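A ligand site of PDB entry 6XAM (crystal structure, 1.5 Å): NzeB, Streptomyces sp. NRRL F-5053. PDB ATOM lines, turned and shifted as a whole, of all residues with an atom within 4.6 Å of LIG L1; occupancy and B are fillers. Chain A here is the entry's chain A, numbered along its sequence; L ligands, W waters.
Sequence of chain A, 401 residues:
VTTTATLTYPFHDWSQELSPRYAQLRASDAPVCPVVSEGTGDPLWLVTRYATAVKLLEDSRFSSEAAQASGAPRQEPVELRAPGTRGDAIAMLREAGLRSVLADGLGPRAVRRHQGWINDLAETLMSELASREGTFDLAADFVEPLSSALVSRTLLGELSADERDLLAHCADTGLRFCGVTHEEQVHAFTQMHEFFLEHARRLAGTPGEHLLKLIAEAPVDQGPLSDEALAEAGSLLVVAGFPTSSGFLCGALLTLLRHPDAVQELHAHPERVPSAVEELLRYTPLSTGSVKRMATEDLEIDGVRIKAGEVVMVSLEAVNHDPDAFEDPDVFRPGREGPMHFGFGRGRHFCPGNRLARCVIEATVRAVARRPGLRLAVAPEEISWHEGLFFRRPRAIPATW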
ATOM      1  N   SER A  64      -6.950  29.189  13.673  1.00  0.00           N
ATOM      2  CA  SER A  64      -8.270  28.581  13.770  1.00  0.00           C
ATOM      3  C   SER A  64      -9.272  29.573  14.314  1.00  0.00           C
ATOM      4  O   SER A  64     -10.381  29.719  13.771  1.00  0.00           O
ATOM      5  CB  SER A  64      -8.213  27.349  14.664  1.00  0.00           C
ATOM      6  OG  SER A  64      -9.535  26.865  14.838  1.00  0.00           O
ATOM      7  N   ILE A  90     -12.804  28.838  24.177  1.00  0.00           N
ATOM      8  CA  ILE A  90     -11.446  28.503  24.584  1.00  0.00           C
ATOM      9  C   ILE A  90     -10.680  29.755  25.024  1.00  0.00           C
ATOM     10  O   ILE A  90      -9.973  29.739  26.038  1.00  0.00           O
ATOM     11  CB  ILE A  90     -10.720  27.715  23.480  1.00  0.00           C
ATOM     12  CG1 ILE A  90     -11.251  26.277  23.401  1.00  0.00           C
ATOM     13  CG2 ILE A  90      -9.204  27.734  23.695  1.00  0.00           C
ATOM     14  CD1 ILE A  90     -10.778  25.498  22.179  1.00  0.00           C
ATOM     15  N   LEU A 102      -9.205  22.316  29.769  1.00  0.00           N
ATOM     16  CA  LEU A 102      -9.825  21.356  28.863  1.00  0.00           C
ATOM     17  C   LEU A 102      -8.968  20.096  28.737  1.00  0.00           C
ATOM     18  O   LEU A 102      -9.403  18.991  29.094  1.00  0.00           O
ATOM     19  CB  LEU A 102     -10.025  21.988  27.487  1.00  0.00           C
ATOM     20  CG  LEU A 102     -11.059  23.110  27.369  1.00  0.00           C
ATOM     21  CD1 LEU A 102     -11.141  23.592  25.932  1.00  0.00           C
ATOM     22  CD2 LEU A 102     -12.420  22.644  27.872  1.00  0.00           C
ATOM     23  N   LEU A 106      -9.357  16.152  30.535  1.00  0.00           N
ATOM     24  CA  LEU A 106      -9.647  15.126  29.541  1.00  0.00           C
ATOM     25  C   LEU A 106      -8.432  14.258  29.224  1.00  0.00           C
ATOM     26  O   LEU A 106      -8.508  13.410  28.333  1.00  0.00           O
ATOM     27  CB  LEU A 106     -10.192  15.772  28.245  1.00  0.00           C
ATOM     28  CG  LEU A 106     -11.439  16.669  28.288  1.00  0.00           C
ATOM     29  CD1 LEU A 106     -11.461  17.614  27.085  1.00  0.00           C
ATOM     30  CD2 LEU A 106     -12.700  15.849  28.313  1.00  0.00           C
ATOM     31  N   LEU A 155     -18.382  15.426  31.248  1.00  0.00           N
ATOM     32  CA  LEU A 155     -18.421  16.766  30.695  1.00  0.00           C
ATOM     33  C   LEU A 155     -19.283  17.729  31.510  1.00  0.00           C
ATOM     34  O   LEU A 155     -18.791  18.759  31.953  1.00  0.00           O
ATOM     35  CB  LEU A 155     -18.869  16.749  29.212  1.00  0.00           C
ATOM     36  CG  LEU A 155     -18.011  15.872  28.297  1.00  0.00           C
ATOM     37  CD1 LEU A 155     -18.431  15.993  26.840  1.00  0.00           C
ATOM     38  CD2 LEU A 155     -16.526  16.158  28.470  1.00  0.00           C
ATOM     39  N   LEU A 236     -19.764  24.775  24.469  1.00  0.00           N
ATOM     40  CA  LEU A 236     -18.590  24.203  23.834  1.00  0.00           C
ATOM     41  C   LEU A 236     -18.529  22.694  24.045  1.00  0.00           C
ATOM     42  O   LEU A 236     -18.261  21.935  23.104  1.00  0.00           O
ATOM     43  CB  LEU A 236     -17.323  24.850  24.392  1.00  0.00           C
ATOM     44  CG  LEU A 236     -16.017  24.102  24.087  1.00  0.00           C
ATOM     45  CD1 LEU A 236     -15.679  24.279  22.632  1.00  0.00           C
ATOM     46  CD2 LEU A 236     -14.851  24.591  24.941  1.00  0.00           C
ATOM     47  N   LEU A 237     -18.765  22.249  25.277  1.00  0.00           N
ATOM     48  CA  LEU A 237     -18.640  20.836  25.573  1.00  0.00           C
ATOM     49  C   LEU A 237     -19.724  20.027  24.871  1.00  0.00           C
ATOM     50  O   LEU A 237     -19.468  18.917  24.390  1.00  0.00           O
ATOM     51  CB  LEU A 237     -18.644  20.616  27.078  1.00  0.00           C
ATOM     52  CG  LEU A 237     -17.443  21.208  27.830  1.00  0.00           C
ATOM     53  CD1 LEU A 237     -17.491  20.876  29.301  1.00  0.00           C
ATOM     54  CD2 LEU A 237     -16.126  20.724  27.206  1.00  0.00           C
ATOM     55  N   ALA A 240     -18.745  20.079  20.983  1.00  0.00           N
ATOM     56  CA  ALA A 240     -17.508  19.377  20.656  1.00  0.00           C
ATOM     57  C   ALA A 240     -17.535  17.914  21.093  1.00  0.00           C
ATOM     58  O   ALA A 240     -16.832  17.086  20.497  1.00  0.00           O
ATOM     59  CB  ALA A 240     -16.303  20.080  21.272  1.00  0.00           C
ATOM     60  N   GLY A 241     -18.328  17.582  22.105  1.00  0.00           N
ATOM     61  CA  GLY A 241     -18.277  16.268  22.714  1.00  0.00           C
ATOM     62  C   GLY A 241     -19.434  15.321  22.436  1.00  0.00           C
ATOM     63  O   GLY A 241     -19.257  14.106  22.481  1.00  0.00           O
ATOM     64  N   THR A 244     -20.123  14.365  18.092  1.00  0.00           N
ATOM     65  CA  THR A 244     -18.890  13.733  17.625  1.00  0.00           C
ATOM     66  C   THR A 244     -18.791  12.310  18.167  1.00  0.00           C
ATOM     67  O   THR A 244     -18.619  11.355  17.412  1.00  0.00           O
ATOM     68  CB  THR A 244     -17.732  14.572  18.153  1.00  0.00           C
ATOM     69  OG1 THR A 244     -17.950  14.827  19.550  1.00  0.00           O
ATOM     70  CG2 THR A 244     -17.658  15.904  17.392  1.00  0.00           C
ATOM     71  N   SER A 245     -18.939  12.152  19.481  1.00  0.00           N
ATOM     72  CA  SER A 245     -18.846  10.818  20.079  1.00  0.00           C
ATOM     73  C   SER A 245     -19.967   9.917  19.589  1.00  0.00           C
ATOM     74  O   SER A 245     -19.719   8.755  19.244  1.00  0.00           O
ATOM     75  CB  SER A 245     -18.881  10.940  21.596  1.00  0.00           C
ATOM     76  OG  SER A 245     -17.780  11.706  22.057  1.00  0.00           O
ATOM     77  N   PHE A 248     -19.364   9.169  15.834  1.00  0.00           N
ATOM     78  CA  PHE A 248     -18.225   8.300  15.561  1.00  0.00           C
ATOM     79  C   PHE A 248     -18.486   6.881  16.034  1.00  0.00           C
ATOM     80  O   PHE A 248     -18.140   5.918  15.331  1.00  0.00           O
ATOM     81  CB  PHE A 248     -16.920   8.821  16.171  1.00  0.00           C
ATOM     82  CG  PHE A 248     -15.747   8.006  15.718  1.00  0.00           C
ATOM     83  CD1 PHE A 248     -15.166   8.261  14.477  1.00  0.00           C
ATOM     84  CD2 PHE A 248     -15.303   6.930  16.465  1.00  0.00           C
ATOM     85  CE1 PHE A 248     -14.148   7.461  14.017  1.00  0.00           C
ATOM     86  CE2 PHE A 248     -14.268   6.138  15.997  1.00  0.00           C
ATOM     87  CZ  PHE A 248     -13.695   6.402  14.775  1.00  0.00           C
ATOM     88  N   LEU A 281     -10.299   5.330  13.523  1.00  0.00           N
ATOM     89  CA  LEU A 281     -10.213   6.780  13.463  1.00  0.00           C
ATOM     90  C   LEU A 281      -9.760   7.269  12.093  1.00  0.00           C
ATOM     91  O   LEU A 281     -10.165   8.349  11.670  1.00  0.00           O
ATOM     92  CB  LEU A 281      -9.278   7.285  14.563  1.00  0.00           C
ATOM     93  CG  LEU A 281      -9.901   7.223  15.970  1.00  0.00           C
ATOM     94  CD1 LEU A 281      -8.844   7.153  17.057  1.00  0.00           C
ATOM     95  CD2 LEU A 281     -10.837   8.418  16.194  1.00  0.00           C
ATOM     96  N   LEU A 286     -16.282  11.020   9.669  1.00  0.00           N
ATOM     97  CA  LEU A 286     -17.115  11.672  10.683  1.00  0.00           C
ATOM     98  C   LEU A 286     -17.733  12.969  10.162  1.00  0.00           C
ATOM     99  O   LEU A 286     -18.900  12.991   9.779  1.00  0.00           O
ATOM    100  CB  LEU A 286     -16.375  11.871  11.999  1.00  0.00           C
ATOM    101  CG  LEU A 286     -17.274  12.441  13.099  1.00  0.00           C
ATOM    102  CD1 LEU A 286     -18.499  11.548  13.357  1.00  0.00           C
ATOM    103  CD2 LEU A 286     -16.468  12.660  14.369  1.00  0.00           C
ATOM    104  N   VAL A 291     -12.090  20.967   8.606  1.00  0.00           N
ATOM    105  CA  VAL A 291     -11.404  21.777   9.599  1.00  0.00           C
ATOM    106  C   VAL A 291     -10.983  23.052   8.820  1.00  0.00           C
ATOM    107  O   VAL A 291     -10.622  22.980   7.644  1.00  0.00           O
ATOM    108  CB  VAL A 291     -10.181  21.005  10.134  1.00  0.00           C
ATOM    109  CG1 VAL A 291      -9.069  21.923  10.597  1.00  0.00           C
ATOM    110  CG2 VAL A 291     -10.606  20.028  11.224  1.00  0.00           C
ATOM    111  N   ARG A 293      -9.064  27.177   8.746  1.00  0.00           N
ATOM    112  CA  ARG A 293      -8.104  28.113   9.318  1.00  0.00           C
ATOM    113  C   ARG A 293      -8.075  29.360   8.446  1.00  0.00           C
ATOM    114  O   ARG A 293      -8.264  29.286   7.226  1.00  0.00           O
ATOM    115  CB  ARG A 293      -6.681  27.545   9.355  1.00  0.00           C
ATOM    116  CG  ARG A 293      -6.540  26.210  10.110  1.00  0.00           C
ATOM    117  CD  ARG A 293      -6.687  26.419  11.583  1.00  0.00           C
ATOM    118  NE  ARG A 293      -6.358  25.216  12.337  1.00  0.00           N
ATOM    119  CZ  ARG A 293      -7.239  24.296  12.710  1.00  0.00           C
ATOM    120  NH1 ARG A 293      -8.527  24.430  12.420  1.00  0.00           N
ATOM    121  NH2 ARG A 293      -6.836  23.239  13.389  1.00  0.00           N
ATOM    122  N   LEU A 316     -10.725  16.127   6.706  1.00  0.00           N
ATOM    123  CA  LEU A 316      -9.992  15.053   7.374  1.00  0.00           C
ATOM    124  C   LEU A 316     -10.252  13.710   6.703  1.00  0.00           C
ATOM    125  O   LEU A 316      -9.353  12.863   6.617  1.00  0.00           O
ATOM    126  CB  LEU A 316     -10.364  14.995   8.860  1.00  0.00           C
ATOM    127  CG  LEU A 316     -10.191  16.330   9.594  1.00  0.00           C
ATOM    128  CD1 LEU A 316     -10.546  16.131  11.042  1.00  0.00           C
ATOM    129  CD2 LEU A 316      -8.772  16.833   9.491  1.00  0.00           C
ATOM    130  N   GLY A 343      -7.848  11.796  12.174  1.00  0.00           N
ATOM    131  CA  GLY A 343      -9.184  11.751  12.764  1.00  0.00           C
ATOM    132  C   GLY A 343      -9.393  12.730  13.910  1.00  0.00           C
ATOM    133  O   GLY A 343     -10.537  13.130  14.190  1.00  0.00           O
ATOM    134  N   PHE A 344      -8.321  13.082  14.621  1.00  0.00           N
ATOM    135  CA  PHE A 344      -8.340  14.068  15.687  1.00  0.00           C
ATOM    136  C   PHE A 344      -7.710  15.384  15.248  1.00  0.00           C
ATOM    137  O   PHE A 344      -7.463  16.246  16.107  1.00  0.00           O
ATOM    138  CB  PHE A 344      -7.609  13.549  16.920  1.00  0.00           C
ATOM    139  CG  PHE A 344      -8.328  12.458  17.671  1.00  0.00           C
ATOM    140  CD1 PHE A 344      -9.662  12.600  18.048  1.00  0.00           C
ATOM    141  CD2 PHE A 344      -7.663  11.283  18.006  1.00  0.00           C
ATOM    142  CE1 PHE A 344     -10.333  11.584  18.745  1.00  0.00           C
ATOM    143  CE2 PHE A 344      -8.324  10.248  18.706  1.00  0.00           C
ATOM    144  CZ  PHE A 344      -9.655  10.407  19.082  1.00  0.00           C
ATOM    145  N   GLY A 345      -7.421  15.550  13.962  1.00  0.00           N
ATOM    146  CA  GLY A 345      -6.771  16.748  13.491  1.00  0.00           C
ATOM    147  C   GLY A 345      -5.260  16.637  13.608  1.00  0.00           C
ATOM    148  O   GLY A 345      -4.689  15.542  13.589  1.00  0.00           O
ATOM    149  N   HIS A 349      -4.385  22.437  17.539  1.00  0.00           N
ATOM    150  CA  HIS A 349      -5.786  22.206  17.895  1.00  0.00           C
ATOM    151  C   HIS A 349      -6.171  20.737  17.890  1.00  0.00           C
ATOM    152  O   HIS A 349      -7.368  20.428  17.896  1.00  0.00           O
ATOM    153  CB  HIS A 349      -6.687  23.030  16.987  1.00  0.00           C
ATOM    154  CG  HIS A 349      -6.421  24.486  17.086  1.00  0.00           C
ATOM    155  ND1 HIS A 349      -6.950  25.273  18.092  1.00  0.00           N
ATOM    156  CD2 HIS A 349      -5.639  25.308  16.340  1.00  0.00           C
ATOM    157  CE1 HIS A 349      -6.521  26.515  17.948  1.00  0.00           C
ATOM    158  NE2 HIS A 349      -5.722  26.560  16.904  1.00  0.00           N
ATOM    159  N   CYS A 351      -7.446  17.307  18.899  1.00  0.00           N
ATOM    160  CA  CYS A 351      -8.579  17.118  19.801  1.00  0.00           C
ATOM    161  C   CYS A 351      -8.107  16.951  21.243  1.00  0.00           C
ATOM    162  O   CYS A 351      -7.390  15.989  21.552  1.00  0.00           O
ATOM    163  CB  CYS A 351      -9.383  15.882  19.402  1.00  0.00           C
ATOM    164  SG  CYS A 351     -10.697  15.535  20.552  1.00  0.00           S
ATOM    165  N   PRO A 352      -8.501  17.848  22.163  1.00  0.00           N
ATOM    166  CA  PRO A 352      -8.105  17.673  23.562  1.00  0.00           C
ATOM    167  C   PRO A 352      -8.878  16.562  24.253  1.00  0.00           C
ATOM    168  O   PRO A 352      -8.451  16.111  25.320  1.00  0.00           O
ATOM    169  CB  PRO A 352      -8.362  19.043  24.190  1.00  0.00           C
ATOM    170  CG  PRO A 352      -9.417  19.663  23.330  1.00  0.00           C
ATOM    171  CD  PRO A 352      -9.204  19.120  21.930  1.00  0.00           C
ATOM    172  N   GLY A 353      -9.987  16.110  23.668  1.00  0.00           N
ATOM    173  CA  GLY A 353     -10.692  14.927  24.141  1.00  0.00           C
ATOM    174  C   GLY A 353     -10.172  13.622  23.579  1.00  0.00           C
ATOM    175  O   GLY A 353     -10.810  12.593  23.786  1.00  0.00           O
ATOM    176  N   ALA A 357     -11.895   9.941  24.057  1.00  0.00           N
ATOM    177  CA  ALA A 357     -12.519   9.352  22.885  1.00  0.00           C
ATOM    178  C   ALA A 357     -11.938   7.978  22.591  1.00  0.00           C
ATOM    179  O   ALA A 357     -12.663   6.999  22.403  1.00  0.00           O
ATOM    180  CB  ALA A 357     -12.392  10.282  21.676  1.00  0.00           C
ATOM    181  N   ILE A 361     -13.999   4.471  22.445  1.00  0.00           N
ATOM    182  CA  ILE A 361     -13.931   3.647  21.238  1.00  0.00           C
ATOM    183  C   ILE A 361     -13.380   2.256  21.565  1.00  0.00           C
ATOM    184  O   ILE A 361     -13.927   1.242  21.124  1.00  0.00           O
ATOM    185  CB  ILE A 361     -13.110   4.361  20.148  1.00  0.00           C
ATOM    186  CG1 ILE A 361     -13.758   5.686  19.750  1.00  0.00           C
ATOM    187  CG2 ILE A 361     -12.997   3.445  18.913  1.00  0.00           C
ATOM    188  CD1 ILE A 361     -12.738   6.677  19.126  1.00  0.00           C
HETATM  189  C1  LIG L   1     -11.185  19.395  18.464  1.00  0.00           C
HETATM  190  C2  LIG L   1     -12.342  15.036  16.643  1.00  0.00           C
HETATM  191  C3  LIG L   1     -14.513  13.869  20.806  1.00  0.00           C
HETATM  192  C4  LIG L   1     -13.451  18.241  22.593  1.00  0.00           C
HETATM  193  C5  LIG L   1     -11.285  18.310  17.632  1.00  0.00           C
HETATM  194  C6  LIG L   1     -10.753  18.246  16.284  1.00  0.00           C
HETATM  195  C7  LIG L   1     -11.103  17.041  15.802  1.00  0.00           C
HETATM  196  C8  LIG L   1     -11.838  16.309  16.798  1.00  0.00           C
HETATM  197  C9  LIG L   1     -10.762  16.495  14.413  1.00  0.00           C
HETATM  198  C10 LIG L   1      -9.909  19.330  15.562  1.00  0.00           C
HETATM  199  C11 LIG L   1     -10.726  20.459  14.955  1.00  0.00           C
HETATM  200  C12 LIG L   1      -9.814  21.486  14.318  1.00  0.00           C
HETATM  201  O1  LIG L   1      -8.615  21.200  14.043  1.00  0.00           O
HETATM  202  O2  LIG L   1     -10.314  22.621  14.063  1.00  0.00           O
HETATM  203  C13 LIG L   1     -13.039  14.342  17.606  1.00  0.00           C
HETATM  204  C14 LIG L   1     -13.531  12.982  17.485  1.00  0.00           C
HETATM  205  C15 LIG L   1     -14.154  12.687  18.644  1.00  0.00           C
HETATM  206  C16 LIG L   1     -14.027  13.823  19.510  1.00  0.00           C
HETATM  207  C17 LIG L   1     -13.371  12.114  16.221  1.00  0.00           C
HETATM  208  C18 LIG L   1     -14.858  11.388  19.071  1.00  0.00           C
HETATM  209  C19 LIG L   1     -14.722  10.230  18.411  1.00  0.00           C
HETATM  210  C20 LIG L   1     -14.399  14.931  21.671  1.00  0.00           C
HETATM  211  C21 LIG L   1     -14.906  14.973  23.023  1.00  0.00           C
HETATM  212  C22 LIG L   1     -14.619  16.196  23.519  1.00  0.00           C
HETATM  213  C23 LIG L   1     -13.923  16.945  22.509  1.00  0.00           C
HETATM  214  C24 LIG L   1     -15.640  13.812  23.742  1.00  0.00           C
HETATM  215  C25 LIG L   1     -14.985  16.656  24.943  1.00  0.00           C
HETATM  216  C26 LIG L   1     -15.343  17.937  25.151  1.00  0.00           C
HETATM  217  C27 LIG L   1     -12.819  18.961  21.598  1.00  0.00           C
HETATM  218  C28 LIG L   1     -12.528  20.389  21.616  1.00  0.00           C
HETATM  219  C29 LIG L   1     -11.910  20.717  20.482  1.00  0.00           C
HETATM  220  C30 LIG L   1     -11.783  19.508  19.695  1.00  0.00           C
HETATM  221  C31 LIG L   1     -12.887  21.335  22.768  1.00  0.00           C
HETATM  222  C32 LIG L   1     -11.434  22.121  20.065  1.00  0.00           C
HETATM  223  C33 LIG L   1      -9.920  22.258  20.140  1.00  0.00           C
HETATM  224  C34 LIG L   1      -9.449  23.537  19.501  1.00  0.00           C
HETATM  225  O3  LIG L   1     -10.151  24.092  18.605  1.00  0.00           O
HETATM  226  O4  LIG L   1      -8.347  23.971  19.918  1.00  0.00           O
HETATM  227  N1  LIG L   1     -11.951  17.116  17.916  1.00  0.00           N
HETATM  228  N2  LIG L   1     -13.340  14.835  18.868  1.00  0.00           N
HETATM  229  N3  LIG L   1     -13.783  16.135  21.394  1.00  0.00           N
HETATM  230  N4  LIG L   1     -12.353  18.450  20.385  1.00  0.00           N
HETATM  231 FE1  LIG L   1     -12.645  16.532  19.733  1.00  0.00          FE
HETATM  232  N1  LG2 L   2     -15.279  20.719  17.460  1.00  0.00           N
HETATM  233  C1  LG2 L   2     -14.552  25.639  16.052  1.00  0.00           C
HETATM  234  O1  LG2 L   2     -14.826  25.961  14.891  1.00  0.00           O
HETATM  235  C2  LG2 L   2     -13.277  24.812  16.329  1.00  0.00           C
HETATM  236  C3  LG2 L   2     -17.728  20.970  16.745  1.00  0.00           C
HETATM  237  C4  LG2 L   2     -15.255  25.706  18.497  1.00  0.00           C
HETATM  238  C5  LG2 L   2     -16.346  24.715  19.044  1.00  0.00           C
HETATM  239  C6  LG2 L   2     -15.819  23.317  19.312  1.00  0.00           C
HETATM  240  C7  LG2 L   2     -13.806  25.191  18.778  1.00  0.00           C
HETATM  241  C8  LG2 L   2     -13.399  23.366  15.689  1.00  0.00           C
HETATM  242  C9  LG2 L   2     -14.428  22.419  16.262  1.00  0.00           C
HETATM  243  C10 LG2 L   2     -14.107  21.416  17.135  1.00  0.00           C
HETATM  244  C11 LG2 L   2     -16.366  21.288  16.764  1.00  0.00           C
HETATM  245  C12 LG2 L   2     -15.845  22.388  15.987  1.00  0.00           C
HETATM  246  C13 LG2 L   2     -16.742  23.132  15.186  1.00  0.00           C
HETATM  247  C14 LG2 L   2     -18.084  22.799  15.166  1.00  0.00           C
HETATM  248  C15 LG2 L   2     -18.572  21.723  15.935  1.00  0.00           C
HETATM  249  N2  LG2 L   2     -12.953  24.794  17.768  1.00  0.00           N
HETATM  250  N3  LG2 L   2     -15.406  26.029  17.054  1.00  0.00           N
HETATM  251  O2  LG2 L   2     -13.390  25.114  19.934  1.00  0.00           O
HETATM  252  N1  LG3 L   3     -13.847  17.042  11.466  1.00  0.00           N
HETATM  253  C1  LG3 L   3     -15.695  22.593  12.065  1.00  0.00           C
HETATM  254  O1  LG3 L   3     -14.789  23.413  12.211  1.00  0.00           O
HETATM  255  C2  LG3 L   3     -15.437  21.137  12.341  1.00  0.00           C
HETATM  256  C3  LG3 L   3     -14.433  15.956  13.735  1.00  0.00           C
HETATM  257  C4  LG3 L   3     -18.129  22.156  11.505  1.00  0.00           C
HETATM  258  C5  LG3 L   3     -19.090  22.679  10.408  1.00  0.00           C
HETATM  259  C6  LG3 L   3     -18.513  22.543   9.002  1.00  0.00           C
HETATM  260  C7  LG3 L   3     -17.638  20.735  11.175  1.00  0.00           C
HETATM  261  C8  LG3 L   3     -13.974  20.684  12.093  1.00  0.00           C
HETATM  262  C9  LG3 L   3     -13.954  19.166  12.128  1.00  0.00           C
HETATM  263  C10 LG3 L   3     -13.722  18.359  11.032  1.00  0.00           C
HETATM  264  C11 LG3 L   3     -14.182  17.004  12.842  1.00  0.00           C
HETATM  265  C12 LG3 L   3     -14.261  18.374  13.279  1.00  0.00           C
HETATM  266  C13 LG3 L   3     -14.591  18.655  14.618  1.00  0.00           C
HETATM  267  C14 LG3 L   3     -14.825  17.615  15.504  1.00  0.00           C
HETATM  268  C15 LG3 L   3     -14.763  16.265  15.051  1.00  0.00           C
HETATM  269  N2  LG3 L   3     -16.382  20.298  11.567  1.00  0.00           N
HETATM  270  N3  LG3 L   3     -16.961  23.062  11.685  1.00  0.00           N
HETATM  271  O2  LG3 L   3     -18.356  19.930  10.561  1.00  0.00           O
HETATM  272  O   HOH W   1     -12.050  23.738  12.291  1.00  0.00           O
HETATM  273  O   HOH W   2      -6.987  22.953  22.003  1.00  0.00           O
HETATM  274  O   HOH W   3      -6.461  19.839  14.732  1.00  0.00           O
HETATM  275  O   HOH W   4     -15.008  18.063  18.828  1.00  0.00           O
HETATM  276  O   HOH W   5     -10.092  26.942  18.679  1.00  0.00           O
HETATM  277  O   HOH W   6      -9.736  24.523  15.969  1.00  0.00           O
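A ring nitrogen (ND1) of His 349 lies within hydrogen-bond range of an oxygen (O4) of LIG L1 (2.6 Å).
NH2 of Arg 293 lies within salt-bridge range of O1 of LIG L1 (2.8 Å).
SG of Cys 351 binds FE1 of LIG L1 (2.3 Å).
O3 of LIG L1 is in hydrogen-bond range of N2 of LG2 L2.
The backbone NH (N) of Cys 351 sits at hydrogen-bond distance from the backbone carbonyl oxygen (O) of Phe 344 (3.0 Å).
The backbone NH (N) of Gly 353 sits close to the side-chain sulfur (SG) of Cys 351 (3.2 Å).
The side-chain hydroxyl of Thr 244 lies within hydrogen-bond range of the backbone carbonyl oxygen of Ala 240.
The backbone carbonyl oxygen of Gly 241 lies close to the side-chain hydroxyl of Thr 244, 3.3 Å away.
O of Gly 241 lies within hydrogen-bond range of OG of Ser 245.
O of Ala 240 lies close to N3 of LIG L1 (3.3 Å).
Residues that only touch LIG L1: Ile 90 (3.6 Å), Leu 155 (3.9 Å), Leu 237 (3.6 Å), Gly 241 (3.6 Å), Thr 244 (3.8 Å), Ser 245 (3.4 Å), Phe 248 (3.4 Å), Leu 286 (3.6 Å), Val 291 (3.5 Å), Leu 316 (3.4 Å), Gly 343 (3.4 Å), Phe 344 (3.4 Å), Gly 345 (3.5 Å), Pro 352 (3.4 Å) and Ala 357 (3.8 Å).
Hydrophobic or aromatic side chains that line LIG L1: Ile 90, Leu 155, Leu 237, Ala 240, Phe 248, Leu 286, Val 291, Leu 316, Phe 344, His 349, Pro 352 and Ala 357.
19 residues have an atom within 4 Å of LIG L1: Ile 90, Leu 155, Leu 237, Ala 240, Gly 241, Thr 244, Ser 245, Phe 248, Leu 286, Val 291, Arg 293, Leu 316, Gly 343, Phe 344, Gly 345, His 349, Cys 351, Pro 352 and Ala 357.
The nearest printed residue that does not touch LIG L1 is Leu 236 (4.1 Å).
Water W3 lies within hydrogen-bond range of an oxygen (O1) of LIG L1 (2.6 Å) and the backbone carbonyl oxygen of His 349 (3.3 Å).
Water W6 lies within hydrogen-bond range of OG of Ser 64 (2.6 Å) and O3 of LIG L1 (2.7 Å).
Water W1 lies within hydrogen-bond range of an oxygen (O2) of LIG L1 and an oxygen (O1) of LG3 L3.
Water W4 bridges O of Ala 240 (2.7 Å) and N1 of LG2 L2 (3.0 Å).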
